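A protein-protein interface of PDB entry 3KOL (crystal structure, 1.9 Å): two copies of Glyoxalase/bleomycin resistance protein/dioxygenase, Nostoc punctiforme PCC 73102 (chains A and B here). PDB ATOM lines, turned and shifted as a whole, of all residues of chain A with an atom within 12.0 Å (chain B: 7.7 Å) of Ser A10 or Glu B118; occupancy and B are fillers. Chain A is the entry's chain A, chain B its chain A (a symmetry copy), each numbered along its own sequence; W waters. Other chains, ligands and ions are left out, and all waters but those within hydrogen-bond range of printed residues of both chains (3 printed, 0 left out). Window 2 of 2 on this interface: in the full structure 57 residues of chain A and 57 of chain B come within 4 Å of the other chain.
Ser A10 touches Val B115 (O to CG1, 3.6 Å). Thr B39 touches Val A11 (O to CB, 3.3 Å). Ile B40 touches Val A11. Val B115 touches Val A11. Leu A12 touches Leu B41. CA of Ala B112 touches CD2 of Leu A12, at 3.98 Å. Leu B41 touches Leu A17.
Water W1 lies within hydrogen-bond range of the guanidinium group of Arg B111 (2.6 Å) and the backbone carbonyl oxygen of Val A11 (2.8 Å). Water W3 lies within hydrogen-bond range of the side-chain carboxylate (OE1) of Glu B118 (2.6 Å) and the backbone carbonyl oxygen (O) of Val A8 (3.0 Å). Water W2 lies within hydrogen-bond range of O of Leu B41, O of Ala A13 and N of Leu A17.
O of Val B115 lies within hydrogen-bond range of ND2 of Asn B119 (2.9 Å).
Of the printed residues of chain B, Ser A10 touches Val B115 (3.6 Å), Glu B118 (2.9 Å) and Asn B119 (2.8 Å). Glu B118 touches just these residues of chain A: Asn A9 (3.2 Å) and Ser A10 (2.9 Å). Of the printed residues of chain A, Ile B40 touches Val A11 (3.8 Å) and Leu A12 (3.0 Å). No residue of chain A comes within 4 Å of Gly B117. No residue of chain A comes within 4 Å of Lys B120. Of the printed residues of chain B, Leu A17 touches Leu B41 (3.6 Å). Printed residues of chain A within 4 Å of Ala B112: Leu A12. Printed residues of chain A within 4 Å of Leu B41: Leu A12 and Leu A17. Printed residues of chain B within 4 Å of Leu A12: Ile B40, Leu B41 and Ala B112. Printed residues of chain A within 4 Å of Val B115: Ser A10 (3.6 Å) and Val A11 (3.8 Å). Val A8 touches none of the printed residues of chain B. The nearest residue of chain A that does not touch Glu B118 is Val A8 (4.3 Å). The nearest printed residue of chain A that does not touch Ala B112 is Leu A17 (5.8 Å).
The side-chain hydroxyl of Ser A10 lies within hydrogen-bond range of the side-chain carboxylate of Glu B118 (2.9 Å). N of Leu A12 sits at hydrogen-bond distance from O of Ile B40, 3.0 Å away. The side-chain amide nitrogen of Asn A9 lies within hydrogen-bond range of the side-chain amide oxygen of Asn B119 (3.5 Å). The backbone carbonyl oxygen (O) of Glu B118 sits close to the side-chain amide oxygen (OD1) of Asn A9. O of Ser A10 lies within hydrogen-bond range of ND2 of Asn B119, 2.8 Å away.
Printed residues of chain A that touch a printed residue of chain B: Asn A9, Ser A10, Val A11, Leu A12 and Leu A17. Of the 14 printed residues of chain B, 7 touch a printed residue of chain A. Printed residues of chain B that touch a printed residue of chain A: Thr B39, Ile B40, Leu B41, Ala B112, Val B115, Glu B118 and Asn B119. Hydrophobic or aromatic side chains of chain B that line the printed part of chain A: Leu B41 and Val B115. Among the printed residues, no Asp or Glu carboxylate lies within 4 Å of a Lys or Arg side-chain nitrogen of the other chain.
No position is printed for both chains. Of the 12 pairs that touch across the chains among the printed residues, none has its exchanged pair printed and touching as well.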
ATOM      1  N   SER A   7     -14.959  27.126 -11.277  1.00  0.00           N
ATOM      2  CA  SER A   7     -15.063  28.155 -12.354  1.00  0.00           C
ATOM      3  C   SER A   7     -15.343  27.512 -13.713  1.00  0.00           C
ATOM      4  O   SER A   7     -15.065  26.329 -13.921  1.00  0.00           O
ATOM      5  CB  SER A   7     -13.765  28.958 -12.433  1.00  0.00           C
ATOM      6  OG  SER A   7     -12.667  28.110 -12.713  1.00  0.00           O
ATOM      7  N   VAL A   8     -15.896  28.300 -14.630  1.00  0.00           N
ATOM      8  CA  VAL A   8     -16.209  27.833 -15.976  1.00  0.00           C
ATOM      9  C   VAL A   8     -15.093  28.303 -16.910  1.00  0.00           C
ATOM     10  O   VAL A   8     -14.772  29.490 -16.943  1.00  0.00           O
ATOM     11  CB  VAL A   8     -17.558  28.416 -16.459  1.00  0.00           C
ATOM     12  CG1 VAL A   8     -17.818  28.016 -17.901  1.00  0.00           C
ATOM     13  CG2 VAL A   8     -18.687  27.922 -15.568  1.00  0.00           C
ATOM     14  N   ASN A   9     -14.502  27.379 -17.661  1.00  0.00           N
ATOM     15  CA  ASN A   9     -13.415  27.734 -18.573  1.00  0.00           C
ATOM     16  C   ASN A   9     -13.895  28.545 -19.767  1.00  0.00           C
ATOM     17  O   ASN A   9     -14.987  28.322 -20.284  1.00  0.00           O
ATOM     18  CB  ASN A   9     -12.705  26.481 -19.093  1.00  0.00           C
ATOM     19  CG  ASN A   9     -12.125  25.632 -17.984  1.00  0.00           C
ATOM     20  OD1 ASN A   9     -11.581  26.149 -17.010  1.00  0.00           O
ATOM     21  ND2 ASN A   9     -12.223  24.318 -18.135  1.00  0.00           N
ATOM     22  N   SER A  10     -13.075  29.494 -20.202  1.00  0.00           N
ATOM     23  CA  SER A  10     -13.423  30.300 -21.358  1.00  0.00           C
ATOM     24  C   SER A  10     -13.303  29.373 -22.566  1.00  0.00           C
ATOM     25  O   SER A  10     -12.463  28.477 -22.584  1.00  0.00           O
ATOM     26  CB  SER A  10     -12.452  31.477 -21.508  1.00  0.00           C
ATOM     27  OG  SER A  10     -12.537  32.349 -20.391  1.00  0.00           O
ATOM     28  N   VAL A  11     -14.162  29.571 -23.556  1.00  0.00           N
ATOM     29  CA  VAL A  11     -14.121  28.755 -24.767  1.00  0.00           C
ATOM     30  C   VAL A  11     -14.388  29.657 -25.953  1.00  0.00           C
ATOM     31  O   VAL A  11     -14.933  30.744 -25.796  1.00  0.00           O
ATOM     32  CB  VAL A  11     -15.189  27.631 -24.751  1.00  0.00           C
ATOM     33  CG1 VAL A  11     -14.948  26.705 -23.574  1.00  0.00           C
ATOM     34  CG2 VAL A  11     -16.594  28.226 -24.695  1.00  0.00           C
ATOM     35  N   LEU A  12     -13.995  29.217 -27.143  1.00  0.00           N
ATOM     36  CA  LEU A  12     -14.245  30.024 -28.325  1.00  0.00           C
ATOM     37  C   LEU A  12     -15.708  29.882 -28.719  1.00  0.00           C
ATOM     38  O   LEU A  12     -16.333  28.843 -28.492  1.00  0.00           O
ATOM     39  CB  LEU A  12     -13.339  29.596 -29.488  1.00  0.00           C
ATOM     40  CG  LEU A  12     -11.853  29.950 -29.349  1.00  0.00           C
ATOM     41  CD1 LEU A  12     -11.102  29.500 -30.586  1.00  0.00           C
ATOM     42  CD2 LEU A  12     -11.695  31.452 -29.173  1.00  0.00           C
ATOM     43  N   ALA A  13     -16.253  30.947 -29.291  1.00  0.00           N
ATOM     44  CA  ALA A  13     -17.639  30.953 -29.720  1.00  0.00           C
ATOM     45  C   ALA A  13     -17.706  30.478 -31.165  1.00  0.00           C
ATOM     46  O   ALA A  13     -16.721  30.553 -31.898  1.00  0.00           O
ATOM     47  CB  ALA A  13     -18.204  32.359 -29.606  1.00  0.00           C
ATOM     48  N   PRO A  14     -18.865  29.957 -31.588  1.00  0.00           N
ATOM     49  CA  PRO A  14     -18.965  29.500 -32.972  1.00  0.00           C
ATOM     50  C   PRO A  14     -18.730  30.687 -33.897  1.00  0.00           C
ATOM     51  O   PRO A  14     -19.313  31.756 -33.702  1.00  0.00           O
ATOM     52  CB  PRO A  14     -20.389  28.956 -33.053  1.00  0.00           C
ATOM     53  CG  PRO A  14     -21.127  29.778 -32.032  1.00  0.00           C
ATOM     54  CD  PRO A  14     -20.152  29.812 -30.886  1.00  0.00           C
ATOM     55  N   ASN A  16     -15.648  32.063 -34.369  1.00  0.00           N
ATOM     56  CA  ASN A  16     -14.317  32.605 -34.089  1.00  0.00           C
ATOM     57  C   ASN A  16     -13.303  31.970 -35.036  1.00  0.00           C
ATOM     58  O   ASN A  16     -12.507  32.671 -35.662  1.00  0.00           O
ATOM     59  CB  ASN A  16     -13.922  32.365 -32.632  1.00  0.00           C
ATOM     60  CG  ASN A  16     -14.725  33.226 -31.664  1.00  0.00           C
ATOM     61  OD1 ASN A  16     -15.509  34.085 -32.079  1.00  0.00           O
ATOM     62  ND2 ASN A  16     -14.525  33.007 -30.375  1.00  0.00           N
ATOM     63  N   LEU A  17     -13.309  30.645 -35.126  1.00  0.00           N
ATOM     64  CA  LEU A  17     -12.432  29.973 -36.076  1.00  0.00           C
ATOM     65  C   LEU A  17     -13.270  30.099 -37.349  1.00  0.00           C
ATOM     66  O   LEU A  17     -14.180  29.304 -37.599  1.00  0.00           O
ATOM     67  CB  LEU A  17     -12.217  28.515 -35.671  1.00  0.00           C
ATOM     68  CG  LEU A  17     -11.468  28.334 -34.341  1.00  0.00           C
ATOM     69  CD1 LEU A  17     -11.034  26.885 -34.200  1.00  0.00           C
ATOM     70  CD2 LEU A  17     -10.235  29.250 -34.295  1.00  0.00           C
ATOM     71  N   THR B  39     -16.749  22.060 -28.270  1.00  0.00           N
ATOM     72  CA  THR B  39     -16.891  22.872 -27.070  1.00  0.00           C
ATOM     73  C   THR B  39     -15.791  23.901 -26.852  1.00  0.00           C
ATOM     74  O   THR B  39     -16.069  25.094 -26.677  1.00  0.00           O
ATOM     75  CB  THR B  39     -17.010  21.974 -25.828  1.00  0.00           C
ATOM     76  OG1 THR B  39     -18.141  21.105 -25.989  1.00  0.00           O
ATOM     77  CG2 THR B  39     -17.204  22.816 -24.567  1.00  0.00           C
ATOM     78  N   ILE B  40     -14.542  23.453 -26.859  1.00  0.00           N
ATOM     79  CA  ILE B  40     -13.426  24.368 -26.643  1.00  0.00           C
ATOM     80  C   ILE B  40     -13.117  25.255 -27.848  1.00  0.00           C
ATOM     81  O   ILE B  40     -13.071  26.474 -27.716  1.00  0.00           O
ATOM     82  CB  ILE B  40     -12.156  23.600 -26.246  1.00  0.00           C
ATOM     83  CG1 ILE B  40     -12.391  22.873 -24.917  1.00  0.00           C
ATOM     84  CG2 ILE B  40     -10.976  24.565 -26.132  1.00  0.00           C
ATOM     85  CD1 ILE B  40     -11.294  21.895 -24.532  1.00  0.00           C
ATOM     86  N   LEU B  41     -12.915  24.656 -29.019  1.00  0.00           N
ATOM     87  CA  LEU B  41     -12.606  25.450 -30.207  1.00  0.00           C
ATOM     88  C   LEU B  41     -13.835  26.128 -30.825  1.00  0.00           C
ATOM     89  O   LEU B  41     -13.710  26.950 -31.734  1.00  0.00           O
ATOM     90  CB  LEU B  41     -11.897  24.585 -31.253  1.00  0.00           C
ATOM     91  CG  LEU B  41     -10.547  23.994 -30.825  1.00  0.00           C
ATOM     92  CD1 LEU B  41      -9.854  23.424 -32.040  1.00  0.00           C
ATOM     93  CD2 LEU B  41      -9.670  25.065 -30.193  1.00  0.00           C
ATOM     94  N   ARG B 111      -7.533  35.871 -27.280  1.00  0.00           N
ATOM     95  CA  ARG B 111      -8.570  35.119 -26.585  1.00  0.00           C
ATOM     96  C   ARG B 111      -8.379  33.627 -26.816  1.00  0.00           C
ATOM     97  O   ARG B 111      -8.541  32.831 -25.901  1.00  0.00           O
ATOM     98  CB  ARG B 111      -9.964  35.547 -27.061  1.00  0.00           C
ATOM     99  CG  ARG B 111     -11.100  34.662 -26.546  1.00  0.00           C
ATOM    100  CD  ARG B 111     -11.002  34.432 -25.043  1.00  0.00           C
ATOM    101  NE  ARG B 111     -11.140  35.670 -24.281  1.00  0.00           N
ATOM    102  CZ  ARG B 111     -12.306  36.220 -23.951  1.00  0.00           C
ATOM    103  NH1 ARG B 111     -13.443  35.637 -24.311  1.00  0.00           N
ATOM    104  NH2 ARG B 111     -12.336  37.357 -23.268  1.00  0.00           N
ATOM    105  N   ALA B 112      -8.029  33.253 -28.045  1.00  0.00           N
ATOM    106  CA  ALA B 112      -7.811  31.848 -28.378  1.00  0.00           C
ATOM    107  C   ALA B 112      -6.674  31.274 -27.542  1.00  0.00           C
ATOM    108  O   ALA B 112      -6.777  30.168 -27.009  1.00  0.00           O
ATOM    109  CB  ALA B 112      -7.495  31.699 -29.868  1.00  0.00           C
ATOM    110  N   VAL B 113      -5.587  32.029 -27.423  1.00  0.00           N
ATOM    111  CA  VAL B 113      -4.444  31.577 -26.634  1.00  0.00           C
ATOM    112  C   VAL B 113      -4.885  31.394 -25.178  1.00  0.00           C
ATOM    113  O   VAL B 113      -4.524  30.414 -24.527  1.00  0.00           O
ATOM    114  CB  VAL B 113      -3.275  32.603 -26.709  1.00  0.00           C
ATOM    115  CG1 VAL B 113      -2.174  32.226 -25.747  1.00  0.00           C
ATOM    116  CG2 VAL B 113      -2.729  32.652 -28.129  1.00  0.00           C
ATOM    117  N   THR B 114      -5.679  32.335 -24.680  1.00  0.00           N
ATOM    118  CA  THR B 114      -6.167  32.269 -23.303  1.00  0.00           C
ATOM    119  C   THR B 114      -7.103  31.067 -23.122  1.00  0.00           C
ATOM    120  O   THR B 114      -7.065  30.391 -22.098  1.00  0.00           O
ATOM    121  CB  THR B 114      -6.903  33.572 -22.922  1.00  0.00           C
ATOM    122  OG1 THR B 114      -6.004  34.683 -23.074  1.00  0.00           O
ATOM    123  CG2 THR B 114      -7.390  33.515 -21.482  1.00  0.00           C
ATOM    124  N   VAL B 115      -7.939  30.805 -24.123  1.00  0.00           N
ATOM    125  CA  VAL B 115      -8.865  29.670 -24.076  1.00  0.00           C
ATOM    126  C   VAL B 115      -8.075  28.373 -23.960  1.00  0.00           C
ATOM    127  O   VAL B 115      -8.406  27.501 -23.160  1.00  0.00           O
ATOM    128  CB  VAL B 115      -9.752  29.634 -25.347  1.00  0.00           C
ATOM    129  CG1 VAL B 115     -10.421  28.266 -25.499  1.00  0.00           C
ATOM    130  CG2 VAL B 115     -10.803  30.734 -25.257  1.00  0.00           C
ATOM    131  N   ILE B 116      -7.021  28.247 -24.763  1.00  0.00           N
ATOM    132  CA  ILE B 116      -6.178  27.056 -24.730  1.00  0.00           C
ATOM    133  C   ILE B 116      -5.589  26.879 -23.330  1.00  0.00           C
ATOM    134  O   ILE B 116      -5.521  25.764 -22.803  1.00  0.00           O
ATOM    135  CB  ILE B 116      -5.028  27.174 -25.749  1.00  0.00           C
ATOM    136  CG1 ILE B 116      -5.598  27.160 -27.171  1.00  0.00           C
ATOM    137  CG2 ILE B 116      -4.025  26.047 -25.541  1.00  0.00           C
ATOM    138  CD1 ILE B 116      -4.582  27.526 -28.242  1.00  0.00           C
ATOM    139  N   GLY B 117      -5.167  27.990 -22.736  1.00  0.00           N
ATOM    140  CA  GLY B 117      -4.589  27.948 -21.404  1.00  0.00           C
ATOM    141  C   GLY B 117      -5.594  27.584 -20.323  1.00  0.00           C
ATOM    142  O   GLY B 117      -5.326  26.723 -19.485  1.00  0.00           O
ATOM    143  N   GLU B 118      -6.752  28.237 -20.331  1.00  0.00           N
ATOM    144  CA  GLU B 118      -7.770  27.957 -19.324  1.00  0.00           C
ATOM    145  C   GLU B 118      -8.270  26.521 -19.389  1.00  0.00           C
ATOM    146  O   GLU B 118      -8.731  25.973 -18.384  1.00  0.00           O
ATOM    147  CB  GLU B 118      -8.947  28.924 -19.465  1.00  0.00           C
ATOM    148  CG  GLU B 118      -8.682  30.278 -18.837  1.00  0.00           C
ATOM    149  CD  GLU B 118      -9.881  31.196 -18.880  1.00  0.00           C
ATOM    150  OE1 GLU B 118     -11.006  30.722 -18.611  1.00  0.00           O
ATOM    151  OE2 GLU B 118      -9.697  32.398 -19.166  1.00  0.00           O
ATOM    152  N   ASN B 119      -8.173  25.907 -20.565  1.00  0.00           N
ATOM    153  CA  ASN B 119      -8.618  24.528 -20.733  1.00  0.00           C
ATOM    154  C   ASN B 119      -7.466  23.543 -20.594  1.00  0.00           C
ATOM    155  O   ASN B 119      -7.581  22.367 -20.944  1.00  0.00           O
ATOM    156  CB  ASN B 119      -9.316  24.370 -22.083  1.00  0.00           C
ATOM    157  CG  ASN B 119     -10.736  24.892 -22.052  1.00  0.00           C
ATOM    158  OD1 ASN B 119     -11.645  24.214 -21.567  1.00  0.00           O
ATOM    159  ND2 ASN B 119     -10.931  26.111 -22.534  1.00  0.00           N
ATOM    160  N   LYS B 120      -6.354  24.049 -20.078  1.00  0.00           N
ATOM    161  CA  LYS B 120      -5.158  23.257 -19.842  1.00  0.00           C
ATOM    162  C   LYS B 120      -4.691  22.415 -21.022  1.00  0.00           C
ATOM    163  O   LYS B 120      -4.298  21.256 -20.866  1.00  0.00           O
ATOM    164  CB  LYS B 120      -5.365  22.381 -18.602  1.00  0.00           C
ATOM    165  CG  LYS B 120      -5.672  23.193 -17.349  1.00  0.00           C
ATOM    166  CD  LYS B 120      -5.760  22.319 -16.106  1.00  0.00           C
ATOM    167  CE  LYS B 120      -6.032  23.156 -14.866  1.00  0.00           C
ATOM    168  NZ  LYS B 120      -7.314  23.907 -14.968  1.00  0.00           N
ATOM    169  N   ILE B 121      -4.737  23.006 -22.210  1.00  0.00           N
ATOM    170  CA  ILE B 121      -4.269  22.320 -23.405  1.00  0.00           C
ATOM    171  C   ILE B 121      -2.812  22.755 -23.589  1.00  0.00           C
ATOM    172  O   ILE B 121      -2.518  23.949 -23.672  1.00  0.00           O
ATOM    173  CB  ILE B 121      -5.098  22.712 -24.648  1.00  0.00           C
ATOM    174  CG1 ILE B 121      -6.522  22.152 -24.520  1.00  0.00           C
ATOM    175  CG2 ILE B 121      -4.424  22.190 -25.910  1.00  0.00           C
ATOM    176  CD1 ILE B 121      -7.462  22.583 -25.633  1.00  0.00           C
HETATM  177  O   HOH W   1     -13.862  33.241 -25.090  1.00  0.00           O
HETATM  178  O   HOH W   2     -14.981  28.814 -33.229  1.00  0.00           O
HETATM  179  O   HOH W   3     -11.936  29.997 -16.238  1.00  0.00           O
